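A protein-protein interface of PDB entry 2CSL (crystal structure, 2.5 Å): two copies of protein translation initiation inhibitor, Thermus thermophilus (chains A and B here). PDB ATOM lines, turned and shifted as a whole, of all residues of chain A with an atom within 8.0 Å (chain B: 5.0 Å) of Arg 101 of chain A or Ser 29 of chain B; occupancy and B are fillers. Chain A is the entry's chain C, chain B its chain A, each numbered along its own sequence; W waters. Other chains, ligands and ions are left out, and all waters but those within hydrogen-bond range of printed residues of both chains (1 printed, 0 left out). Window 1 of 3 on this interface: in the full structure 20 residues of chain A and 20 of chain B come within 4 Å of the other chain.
The backbone carbonyl oxygen (O) of Pro 99 of chain A sits at hydrogen-bond distance from the backbone NH (N) of Ala 17 of chain B (3.2 Å). The side-chain hydroxyl (OG) of Ser 29 of chain B is in hydrogen-bond range of the backbone NH (N) of Arg 101 of chain A. N of Gly 30 of chain B lies within hydrogen-bond range of O of Arg 101 of chain A (2.7 Å). The side-chain carboxylate (OE2) of Glu 116 of chain B sits at hydrogen-bond distance from the backbone NH (N) of Thr 103 of chain A (3.3 Å).
O of Ala 17 of chain B sits at hydrogen-bond distance from OG of Ser 29 of chain B, 2.5 Å away. The backbone carbonyl oxygen of Gln 18 of chain B is in hydrogen-bond range of the backbone NH of Ser 29 of chain B. O of Val 71 of chain A lies within hydrogen-bond range of N of Ala 100 of chain A, at 2.8 Å. The side-chain hydroxyl (OH) of Tyr 90 of chain A is in hydrogen-bond range of the side-chain hydroxyl (OG1) of Thr 73 of chain A, at 2.9 Å. The backbone NH (N) of Cys 75 of chain A sits at hydrogen-bond distance from the backbone carbonyl oxygen (O) of Ala 102 of chain A (2.8 Å). The backbone carbonyl oxygen (O) of Cys 75 of chain A sits at hydrogen-bond distance from the backbone NH (N) of Val 104 of chain A (2.9 Å).
Phe 27 of chain B touches Val 71 of chain A. Gln 72 of chain A touches Phe 27 of chain B (NE2 to CD1, 3.7 Å). OD1 of Asn 87 of chain A touches CD of Pro 15 of chain B, at 3.5 Å. Pro 15 of chain B touches Ala 91 of chain A. CB of Tyr 98 of chain A touches O of Pro 15 of chain B (3.1 Å). Tyr 98 of chain A touches Tyr 16 of chain B. O of Pro 99 of chain A touches CA of Tyr 16 of chain B, 3.4 Å away. CA of Ala 100 of chain A touches O of Ala 17 of chain B, 3.8 Å away. Ser 29 of chain B touches Ala 100 of chain A (OG to CA, 3.2 Å). CA of Ala 102 of chain A touches OE2 of Glu 116 of chain B (3.5 Å).
Of the printed residues of chain B, Val 71 of chain A touches Phe 27. Of the printed residues of chain B, Ala 91 of chain A touches Pro 15. Printed residues of chain B within 4 Å of Ala 100 of chain A: Ala 17, Phe 27 and Ser 29. Of chain B, only Tyr 16 (3.5 Å), Ser 29 (2.8 Å) and Gly 30 (2.7 Å) come within 4 Å of Arg 101 of chain A. Ala 118 of chain A touches none of the printed residues of chain B. Of the printed residues of chain A, Tyr 16 of chain B touches Tyr 98 (3.2 Å), Pro 99 (3.4 Å) and Arg 101 (3.5 Å). Of chain A, only Ala 100 (3.2 Å) and Arg 101 (2.8 Å) come within 4 Å of Ser 29 of chain B. The nearest printed residue of chain B that does not touch Val 104 of chain A is Gly 30 of chain B (7.7 Å).
Among the printed residues, 19 pairs touch across the chains. Among the printed residues, no Asp or Glu carboxylate lies within 4 Å of a Lys or Arg side-chain nitrogen of the other chain.
2 positions are printed for both chains.
Water W1 lies within hydrogen-bond range of OH of Tyr 90 of chain A (2.7 Å), O of Pro 99 of chain A (2.8 Å) and O of Pro 15 of chain B (2.9 Å).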
ATOM      1  N   VAL A  71      16.021   2.579  -3.707  1.00  0.00           N
ATOM      2  CA  VAL A  71      16.217   1.711  -2.552  1.00  0.00           C
ATOM      3  C   VAL A  71      15.673   2.297  -1.251  1.00  0.00           C
ATOM      4  O   VAL A  71      15.445   1.573  -0.284  1.00  0.00           O
ATOM      5  CB  VAL A  71      17.711   1.378  -2.357  1.00  0.00           C
ATOM      6  CG1 VAL A  71      18.235   0.676  -3.587  1.00  0.00           C
ATOM      7  CG2 VAL A  71      18.513   2.651  -2.091  1.00  0.00           C
ATOM      8  N   GLN A  72      15.446   3.604  -1.231  1.00  0.00           N
ATOM      9  CA  GLN A  72      14.948   4.249  -0.022  1.00  0.00           C
ATOM     10  C   GLN A  72      14.200   5.551  -0.292  1.00  0.00           C
ATOM     11  O   GLN A  72      14.596   6.345  -1.141  1.00  0.00           O
ATOM     12  CB  GLN A  72      16.126   4.535   0.911  1.00  0.00           C
ATOM     13  CG  GLN A  72      15.787   5.324   2.148  1.00  0.00           C
ATOM     14  CD  GLN A  72      16.971   6.129   2.654  1.00  0.00           C
ATOM     15  OE1 GLN A  72      17.352   7.136   2.054  1.00  0.00           O
ATOM     16  NE2 GLN A  72      17.564   5.684   3.755  1.00  0.00           N
ATOM     17  N   THR A  73      13.115   5.762   0.439  1.00  0.00           N
ATOM     18  CA  THR A  73      12.337   6.981   0.308  1.00  0.00           C
ATOM     19  C   THR A  73      12.008   7.507   1.691  1.00  0.00           C
ATOM     20  O   THR A  73      11.789   6.735   2.636  1.00  0.00           O
ATOM     21  CB  THR A  73      10.987   6.774  -0.409  1.00  0.00           C
ATOM     22  OG1 THR A  73      10.153   5.936   0.394  1.00  0.00           O
ATOM     23  CG2 THR A  73      11.177   6.174  -1.795  1.00  0.00           C
ATOM     24  N   THR A  74      11.979   8.829   1.799  1.00  0.00           N
ATOM     25  CA  THR A  74      11.647   9.496   3.045  1.00  0.00           C
ATOM     26  C   THR A  74      10.384  10.281   2.693  1.00  0.00           C
ATOM     27  O   THR A  74      10.423  11.242   1.921  1.00  0.00           O
ATOM     28  CB  THR A  74      12.816  10.416   3.482  1.00  0.00           C
ATOM     29  OG1 THR A  74      13.985   9.614   3.700  1.00  0.00           O
ATOM     30  CG2 THR A  74      12.494  11.139   4.766  1.00  0.00           C
ATOM     31  N   CYS A  75       9.252   9.845   3.227  1.00  0.00           N
ATOM     32  CA  CYS A  75       7.986  10.490   2.901  1.00  0.00           C
ATOM     33  C   CYS A  75       7.417  11.360   4.006  1.00  0.00           C
ATOM     34  O   CYS A  75       7.158  10.891   5.116  1.00  0.00           O
ATOM     35  CB  CYS A  75       6.968   9.422   2.499  1.00  0.00           C
ATOM     36  SG  CYS A  75       7.629   8.257   1.291  1.00  0.00           S
ATOM     37  N   MET A  80      -1.465  12.870   8.560  1.00  0.00           N
ATOM     38  CA  MET A  80      -1.526  11.411   8.465  1.00  0.00           C
ATOM     39  C   MET A  80      -2.843  10.864   7.894  1.00  0.00           C
ATOM     40  O   MET A  80      -2.873   9.762   7.351  1.00  0.00           O
ATOM     41  CB  MET A  80      -1.255  10.801   9.843  1.00  0.00           C
ATOM     42  CG  MET A  80      -0.520   9.454   9.834  1.00  0.00           C
ATOM     43  SD  MET A  80       1.330   9.478   9.174  1.00  0.00           S
ATOM     44  CE  MET A  80       1.140   8.191   7.764  1.00  0.00           C
ATOM     45  N   PHE A  83      -2.556   9.450   4.473  1.00  0.00           N
ATOM     46  CA  PHE A  83      -1.760   8.277   4.114  1.00  0.00           C
ATOM     47  C   PHE A  83      -2.421   7.353   3.086  1.00  0.00           C
ATOM     48  O   PHE A  83      -1.802   7.005   2.075  1.00  0.00           O
ATOM     49  CB  PHE A  83      -1.387   7.456   5.350  1.00  0.00           C
ATOM     50  CG  PHE A  83      -0.431   6.338   5.052  1.00  0.00           C
ATOM     51  CD1 PHE A  83       0.908   6.602   4.795  1.00  0.00           C
ATOM     52  CD2 PHE A  83      -0.881   5.019   4.974  1.00  0.00           C
ATOM     53  CE1 PHE A  83       1.788   5.568   4.460  1.00  0.00           C
ATOM     54  CE2 PHE A  83      -0.013   3.977   4.639  1.00  0.00           C
ATOM     55  CZ  PHE A  83       1.327   4.254   4.382  1.00  0.00           C
ATOM     56  N   PHE A  86      -2.205   8.762  -0.294  1.00  0.00           N
ATOM     57  CA  PHE A  86      -0.794   8.845  -0.622  1.00  0.00           C
ATOM     58  C   PHE A  86      -0.257   7.471  -1.025  1.00  0.00           C
ATOM     59  O   PHE A  86       0.302   7.300  -2.114  1.00  0.00           O
ATOM     60  CB  PHE A  86       0.002   9.365   0.581  1.00  0.00           C
ATOM     61  CG  PHE A  86       1.488   9.204   0.431  1.00  0.00           C
ATOM     62  CD1 PHE A  86       2.182   8.269   1.195  1.00  0.00           C
ATOM     63  CD2 PHE A  86       2.189   9.964  -0.498  1.00  0.00           C
ATOM     64  CE1 PHE A  86       3.557   8.091   1.031  1.00  0.00           C
ATOM     65  CE2 PHE A  86       3.564   9.790  -0.668  1.00  0.00           C
ATOM     66  CZ  PHE A  86       4.247   8.853   0.098  1.00  0.00           C
ATOM     67  N   ASN A  87      -0.435   6.499  -0.135  1.00  0.00           N
ATOM     68  CA  ASN A  87       0.040   5.139  -0.361  1.00  0.00           C
ATOM     69  C   ASN A  87      -0.491   4.554  -1.676  1.00  0.00           C
ATOM     70  O   ASN A  87       0.257   3.928  -2.429  1.00  0.00           O
ATOM     71  CB  ASN A  87      -0.362   4.272   0.836  1.00  0.00           C
ATOM     72  CG  ASN A  87       0.532   3.055   1.011  1.00  0.00           C
ATOM     73  OD1 ASN A  87       1.731   3.107   0.745  1.00  0.00           O
ATOM     74  ND2 ASN A  87      -0.045   1.960   1.489  1.00  0.00           N
ATOM     75  N   GLU A  88      -1.774   4.774  -1.957  1.00  0.00           N
ATOM     76  CA  GLU A  88      -2.393   4.265  -3.178  1.00  0.00           C
ATOM     77  C   GLU A  88      -1.635   4.709  -4.426  1.00  0.00           C
ATOM     78  O   GLU A  88      -1.223   3.889  -5.244  1.00  0.00           O
ATOM     79  CB  GLU A  88      -3.844   4.739  -3.278  1.00  0.00           C
ATOM     80  CG  GLU A  88      -4.569   4.236  -4.527  1.00  0.00           C
ATOM     81  CD  GLU A  88      -5.959   4.846  -4.703  1.00  0.00           C
ATOM     82  OE1 GLU A  88      -6.805   4.710  -3.786  1.00  0.00           O
ATOM     83  OE2 GLU A  88      -6.203   5.461  -5.767  1.00  0.00           O
ATOM     84  N   TYR A  90       1.298   6.066  -4.528  1.00  0.00           N
ATOM     85  CA  TYR A  90       2.678   5.617  -4.321  1.00  0.00           C
ATOM     86  C   TYR A  90       2.914   4.197  -4.858  1.00  0.00           C
ATOM     87  O   TYR A  90       3.897   3.937  -5.556  1.00  0.00           O
ATOM     88  CB  TYR A  90       3.002   5.666  -2.825  1.00  0.00           C
ATOM     89  CG  TYR A  90       4.439   5.356  -2.458  1.00  0.00           C
ATOM     90  CD1 TYR A  90       5.387   6.374  -2.345  1.00  0.00           C
ATOM     91  CD2 TYR A  90       4.841   4.045  -2.194  1.00  0.00           C
ATOM     92  CE1 TYR A  90       6.700   6.093  -1.970  1.00  0.00           C
ATOM     93  CE2 TYR A  90       6.144   3.757  -1.822  1.00  0.00           C
ATOM     94  CZ  TYR A  90       7.068   4.784  -1.710  1.00  0.00           C
ATOM     95  OH  TYR A  90       8.354   4.500  -1.332  1.00  0.00           O
ATOM     96  N   ALA A  91       2.010   3.287  -4.523  1.00  0.00           N
ATOM     97  CA  ALA A  91       2.114   1.898  -4.976  1.00  0.00           C
ATOM     98  C   ALA A  91       2.106   1.755  -6.496  1.00  0.00           C
ATOM     99  O   ALA A  91       2.548   0.746  -7.025  1.00  0.00           O
ATOM    100  CB  ALA A  91       0.980   1.065  -4.379  1.00  0.00           C
ATOM    101  N   PHE A  94       6.042   2.246  -7.784  1.00  0.00           N
ATOM    102  CA  PHE A  94       7.126   1.406  -7.321  1.00  0.00           C
ATOM    103  C   PHE A  94       6.936  -0.078  -7.614  1.00  0.00           C
ATOM    104  O   PHE A  94       5.820  -0.556  -7.782  1.00  0.00           O
ATOM    105  CB  PHE A  94       7.396   1.701  -5.849  1.00  0.00           C
ATOM    106  CG  PHE A  94       7.926   3.097  -5.622  1.00  0.00           C
ATOM    107  CD1 PHE A  94       7.093   4.114  -5.165  1.00  0.00           C
ATOM    108  CD2 PHE A  94       9.244   3.410  -5.940  1.00  0.00           C
ATOM    109  CE1 PHE A  94       7.570   5.420  -5.035  1.00  0.00           C
ATOM    110  CE2 PHE A  94       9.724   4.703  -5.815  1.00  0.00           C
ATOM    111  CZ  PHE A  94       8.891   5.711  -5.363  1.00  0.00           C
ATOM    112  N   TYR A  98      10.421  -3.497  -3.402  1.00  0.00           N
ATOM    113  CA  TYR A  98      10.010  -2.142  -3.083  1.00  0.00           C
ATOM    114  C   TYR A  98      11.087  -1.430  -2.286  1.00  0.00           C
ATOM    115  O   TYR A  98      11.888  -2.068  -1.608  1.00  0.00           O
ATOM    116  CB  TYR A  98       8.708  -2.155  -2.289  1.00  0.00           C
ATOM    117  CG  TYR A  98       7.502  -2.593  -3.085  1.00  0.00           C
ATOM    118  CD1 TYR A  98       6.798  -3.746  -2.739  1.00  0.00           C
ATOM    119  CD2 TYR A  98       7.049  -1.842  -4.174  1.00  0.00           C
ATOM    120  CE1 TYR A  98       5.671  -4.141  -3.451  1.00  0.00           C
ATOM    121  CE2 TYR A  98       5.925  -2.232  -4.898  1.00  0.00           C
ATOM    122  CZ  TYR A  98       5.240  -3.379  -4.526  1.00  0.00           C
ATOM    123  OH  TYR A  98       4.114  -3.750  -5.216  1.00  0.00           O
ATOM    124  N   PRO A  99      11.117  -0.089  -2.354  1.00  0.00           N
ATOM    125  CA  PRO A  99      12.116   0.683  -1.619  1.00  0.00           C
ATOM    126  C   PRO A  99      11.857   0.570  -0.127  1.00  0.00           C
ATOM    127  O   PRO A  99      10.754   0.221   0.286  1.00  0.00           O
ATOM    128  CB  PRO A  99      11.887   2.112  -2.121  1.00  0.00           C
ATOM    129  CG  PRO A  99      11.283   1.915  -3.486  1.00  0.00           C
ATOM    130  CD  PRO A  99      10.316   0.797  -3.215  1.00  0.00           C
ATOM    131  N   ALA A 100      12.884   0.827   0.676  1.00  0.00           N
ATOM    132  CA  ALA A 100      12.721   0.815   2.122  1.00  0.00           C
ATOM    133  C   ALA A 100      12.002   2.141   2.319  1.00  0.00           C
ATOM    134  O   ALA A 100      12.203   3.066   1.537  1.00  0.00           O
ATOM    135  CB  ALA A 100      14.079   0.829   2.813  1.00  0.00           C
ATOM    136  N   ARG A 101      11.171   2.263   3.344  1.00  0.00           N
ATOM    137  CA  ARG A 101      10.452   3.515   3.501  1.00  0.00           C
ATOM    138  C   ARG A 101      10.257   3.968   4.930  1.00  0.00           C
ATOM    139  O   ARG A 101      10.168   3.148   5.846  1.00  0.00           O
ATOM    140  CB  ARG A 101       9.082   3.397   2.821  1.00  0.00           C
ATOM    141  CG  ARG A 101       8.338   4.714   2.648  1.00  0.00           C
ATOM    142  CD  ARG A 101       7.016   4.523   1.921  1.00  0.00           C
ATOM    143  NE  ARG A 101       6.097   3.684   2.688  1.00  0.00           N
ATOM    144  CZ  ARG A 101       4.900   3.298   2.260  1.00  0.00           C
ATOM    145  NH1 ARG A 101       4.468   3.674   1.065  1.00  0.00           N
ATOM    146  NH2 ARG A 101       4.131   2.536   3.028  1.00  0.00           N
ATOM    147  N   ALA A 102      10.206   5.290   5.098  1.00  0.00           N
ATOM    148  CA  ALA A 102       9.957   5.938   6.386  1.00  0.00           C
ATOM    149  C   ALA A 102       8.915   7.001   6.050  1.00  0.00           C
ATOM    150  O   ALA A 102       9.116   7.812   5.143  1.00  0.00           O
ATOM    151  CB  ALA A 102      11.219   6.592   6.937  1.00  0.00           C
ATOM    152  N   THR A 103       7.794   6.978   6.761  1.00  0.00           N
ATOM    153  CA  THR A 103       6.714   7.927   6.525  1.00  0.00           C
ATOM    154  C   THR A 103       6.411   8.658   7.816  1.00  0.00           C
ATOM    155  O   THR A 103       6.390   8.048   8.886  1.00  0.00           O
ATOM    156  CB  THR A 103       5.433   7.205   6.041  1.00  0.00           C
ATOM    157  OG1 THR A 103       5.718   6.483   4.836  1.00  0.00           O
ATOM    158  CG2 THR A 103       4.322   8.210   5.766  1.00  0.00           C
ATOM    159  N   VAL A 104       6.157   9.958   7.707  1.00  0.00           N
ATOM    160  CA  VAL A 104       5.872  10.785   8.872  1.00  0.00           C
ATOM    161  C   VAL A 104       4.985  11.987   8.520  1.00  0.00           C
ATOM    162  O   VAL A 104       4.925  12.432   7.366  1.00  0.00           O
ATOM    163  CB  VAL A 104       7.197  11.323   9.495  1.00  0.00           C
ATOM    164  CG1 VAL A 104       6.897  12.327  10.573  1.00  0.00           C
ATOM    165  CG2 VAL A 104       8.014  10.188  10.080  1.00  0.00           C
ATOM    166  N   VAL A 117       8.511  14.017  -0.957  1.00  0.00           N
ATOM    167  CA  VAL A 117       9.195  12.733  -0.948  1.00  0.00           C
ATOM    168  C   VAL A 117      10.599  12.843  -1.514  1.00  0.00           C
ATOM    169  O   VAL A 117      10.806  13.341  -2.619  1.00  0.00           O
ATOM    170  CB  VAL A 117       8.431  11.655  -1.753  1.00  0.00           C
ATOM    171  CG1 VAL A 117       9.181  10.333  -1.683  1.00  0.00           C
ATOM    172  CG2 VAL A 117       7.026  11.478  -1.197  1.00  0.00           C
ATOM    173  N   ALA A 118      11.564  12.391  -0.722  1.00  0.00           N
ATOM    174  CA  ALA A 118      12.963  12.386  -1.117  1.00  0.00           C
ATOM    175  C   ALA A 118      13.327  10.915  -1.221  1.00  0.00           C
ATOM    176  O   ALA A 118      12.704  10.072  -0.568  1.00  0.00           O
ATOM    177  CB  ALA A 118      13.826  13.071  -0.057  1.00  0.00           C
ATOM    178  N   PRO B  15       3.571  -1.286  -0.431  1.00  0.00           N
ATOM    179  CA  PRO B  15       4.555  -0.895  -1.449  1.00  0.00           C
ATOM    180  C   PRO B  15       5.982  -0.674  -0.937  1.00  0.00           C
ATOM    181  O   PRO B  15       6.713   0.142  -1.490  1.00  0.00           O
ATOM    182  CB  PRO B  15       3.976   0.408  -2.014  1.00  0.00           C
ATOM    183  CG  PRO B  15       2.542   0.437  -1.540  1.00  0.00           C
ATOM    184  CD  PRO B  15       2.610  -0.200  -0.194  1.00  0.00           C
ATOM    185  N   TYR B  16       6.383  -1.386   0.106  1.00  0.00           N
ATOM    186  CA  TYR B  16       7.727  -1.207   0.647  1.00  0.00           C
ATOM    187  C   TYR B  16       8.295  -2.525   1.140  1.00  0.00           C
ATOM    188  O   TYR B  16       7.569  -3.503   1.271  1.00  0.00           O
ATOM    189  CB  TYR B  16       7.692  -0.212   1.808  1.00  0.00           C
ATOM    190  CG  TYR B  16       6.922  -0.718   3.009  1.00  0.00           C
ATOM    191  CD1 TYR B  16       7.580  -1.233   4.118  1.00  0.00           C
ATOM    192  CD2 TYR B  16       5.537  -0.715   3.019  1.00  0.00           C
ATOM    193  CE1 TYR B  16       6.873  -1.737   5.207  1.00  0.00           C
ATOM    194  CE2 TYR B  16       4.822  -1.221   4.102  1.00  0.00           C
ATOM    195  CZ  TYR B  16       5.497  -1.731   5.190  1.00  0.00           C
ATOM    196  OH  TYR B  16       4.788  -2.262   6.241  1.00  0.00           O
ATOM    197  N   ALA B  17       9.596  -2.540   1.406  1.00  0.00           N
ATOM    198  CA  ALA B  17      10.261  -3.734   1.920  1.00  0.00           C
ATOM    199  C   ALA B  17      10.777  -3.389   3.311  1.00  0.00           C
ATOM    200  O   ALA B  17      11.019  -2.213   3.602  1.00  0.00           O
ATOM    201  CB  ALA B  17      11.423  -4.126   1.012  1.00  0.00           C
ATOM    202  N   GLN B  18      10.929  -4.392   4.175  1.00  0.00           N
ATOM    203  CA  GLN B  18      11.437  -4.145   5.523  1.00  0.00           C
ATOM    204  C   GLN B  18      12.821  -3.517   5.403  1.00  0.00           C
ATOM    205  O   GLN B  18      13.225  -2.703   6.249  1.00  0.00           O
ATOM    206  CB  GLN B  18      11.522  -5.447   6.316  1.00  0.00           C
ATOM    207  CG  GLN B  18      10.167  -6.092   6.560  1.00  0.00           C
ATOM    208  CD  GLN B  18      10.288  -7.470   7.159  1.00  0.00           C
ATOM    209  OE1 GLN B  18      11.003  -8.323   6.631  1.00  0.00           O
ATOM    210  NE2 GLN B  18       9.587  -7.701   8.263  1.00  0.00           N
ATOM    211  N   ALA B  19      13.531  -3.894   4.339  1.00  0.00           N
ATOM    212  CA  ALA B  19      14.857  -3.364   4.067  1.00  0.00           C
ATOM    213  C   ALA B  19      15.319  -3.766   2.673  1.00  0.00           C
ATOM    214  O   ALA B  19      14.843  -4.744   2.102  1.00  0.00           O
ATOM    215  CB  ALA B  19      15.853  -3.866   5.106  1.00  0.00           C
ATOM    216  N   PHE B  27      19.385  -0.596   3.587  1.00  0.00           N
ATOM    217  CA  PHE B  27      18.481   0.509   3.889  1.00  0.00           C
ATOM    218  C   PHE B  27      17.274  -0.074   4.617  1.00  0.00           C
ATOM    219  O   PHE B  27      16.510  -0.845   4.044  1.00  0.00           O
ATOM    220  CB  PHE B  27      18.052   1.204   2.595  1.00  0.00           C
ATOM    221  CG  PHE B  27      19.191   1.817   1.839  1.00  0.00           C
ATOM    222  CD1 PHE B  27      19.597   3.125   2.099  1.00  0.00           C
ATOM    223  CD2 PHE B  27      19.900   1.067   0.900  1.00  0.00           C
ATOM    224  CE1 PHE B  27      20.694   3.674   1.442  1.00  0.00           C
ATOM    225  CE2 PHE B  27      21.001   1.604   0.235  1.00  0.00           C
ATOM    226  CZ  PHE B  27      21.401   2.914   0.508  1.00  0.00           C
ATOM    227  N   VAL B  28      17.119   0.289   5.886  1.00  0.00           N
ATOM    228  CA  VAL B  28      16.020  -0.220   6.703  1.00  0.00           C
ATOM    229  C   VAL B  28      14.835   0.742   6.803  1.00  0.00           C
ATOM    230  O   VAL B  28      15.009   1.933   7.048  1.00  0.00           O
ATOM    231  CB  VAL B  28      16.507  -0.531   8.118  1.00  0.00           C
ATOM    232  CG1 VAL B  28      15.409  -1.200   8.911  1.00  0.00           C
ATOM    233  CG2 VAL B  28      17.727  -1.403   8.047  1.00  0.00           C
ATOM    234  N   SER B  29      13.632   0.209   6.616  1.00  0.00           N
ATOM    235  CA  SER B  29      12.418   1.008   6.683  1.00  0.00           C
ATOM    236  C   SER B  29      12.174   1.501   8.096  1.00  0.00           C
ATOM    237  O   SER B  29      12.687   0.925   9.063  1.00  0.00           O
ATOM    238  CB  SER B  29      11.217   0.180   6.220  1.00  0.00           C
ATOM    239  OG  SER B  29      11.306  -0.108   4.836  1.00  0.00           O
ATOM    240  N   GLY B  30      11.394   2.572   8.216  1.00  0.00           N
ATOM    241  CA  GLY B  30      11.086   3.098   9.530  1.00  0.00           C
ATOM    242  C   GLY B  30      10.342   2.036  10.326  1.00  0.00           C
ATOM    243  O   GLY B  30       9.309   1.531   9.896  1.00  0.00           O
ATOM    244  N   GLN B  31      10.874   1.676  11.484  1.00  0.00           N
ATOM    245  CA  GLN B  31      10.235   0.668  12.307  1.00  0.00           C
ATOM    246  C   GLN B  31       9.433   1.333  13.416  1.00  0.00           C
ATOM    247  O   GLN B  31       9.865   2.348  13.982  1.00  0.00           O
ATOM    248  CB  GLN B  31      11.293  -0.263  12.912  1.00  0.00           C
ATOM    249  CG  GLN B  31      12.092  -1.036  11.882  1.00  0.00           C
ATOM    250  CD  GLN B  31      11.212  -1.931  11.027  1.00  0.00           C
ATOM    251  OE1 GLN B  31      11.196  -1.823   9.797  1.00  0.00           O
ATOM    252  NE2 GLN B  31      10.475  -2.823  11.675  1.00  0.00           N
ATOM    253  N   LEU B  56      14.290  -3.475  14.378  1.00  0.00           N
ATOM    254  CA  LEU B  56      15.488  -3.088  13.629  1.00  0.00           C
ATOM    255  C   LEU B  56      16.479  -4.256  13.622  1.00  0.00           C
ATOM    256  O   LEU B  56      16.981  -4.665  12.571  1.00  0.00           O
ATOM    257  CB  LEU B  56      16.151  -1.860  14.278  1.00  0.00           C
ATOM    258  CG  LEU B  56      15.440  -0.502  14.192  1.00  0.00           C
ATOM    259  CD1 LEU B  56      16.064   0.505  15.156  1.00  0.00           C
ATOM    260  CD2 LEU B  56      15.526   0.005  12.772  1.00  0.00           C
ATOM    261  N   GLU B 116       9.495   6.079  15.803  1.00  0.00           N
ATOM    262  CA  GLU B 116       9.748   5.476  14.506  1.00  0.00           C
ATOM    263  C   GLU B 116      11.223   5.689  14.244  1.00  0.00           C
ATOM    264  O   GLU B 116      11.704   6.819  14.292  1.00  0.00           O
ATOM    265  CB  GLU B 116       8.955   6.143  13.380  1.00  0.00           C
ATOM    266  CG  GLU B 116       9.087   5.374  12.048  1.00  0.00           C
ATOM    267  CD  GLU B 116       8.367   6.033  10.880  1.00  0.00           C
ATOM    268  OE1 GLU B 116       7.293   6.625  11.090  1.00  0.00           O
ATOM    269  OE2 GLU B 116       8.870   5.940   9.743  1.00  0.00           O
ATOM    270  N   VAL B 117      11.940   4.606  13.982  1.00  0.00           N
ATOM    271  CA  VAL B 117      13.359   4.706  13.708  1.00  0.00           C
ATOM    272  C   VAL B 117      13.701   4.017  12.417  1.00  0.00           C
ATOM    273  O   VAL B 117      13.320   2.869  12.199  1.00  0.00           O
ATOM    274  CB  VAL B 117      14.214   4.083  14.821  1.00  0.00           C
ATOM    275  CG1 VAL B 117      15.676   4.060  14.387  1.00  0.00           C
ATOM    276  CG2 VAL B 117      14.059   4.890  16.101  1.00  0.00           C
ATOM    277  N   ALA B 118      14.408   4.738  11.556  1.00  0.00           N
ATOM    278  CA  ALA B 118      14.843   4.210  10.274  1.00  0.00           C
ATOM    279  C   ALA B 118      16.364   4.247  10.332  1.00  0.00           C
ATOM    280  O   ALA B 118      16.949   5.026  11.099  1.00  0.00           O
ATOM    281  CB  ALA B 118      14.334   5.091   9.148  1.00  0.00           C
HETATM  282  O   HOH W   1       8.760   1.970  -0.518  1.00  0.00           O
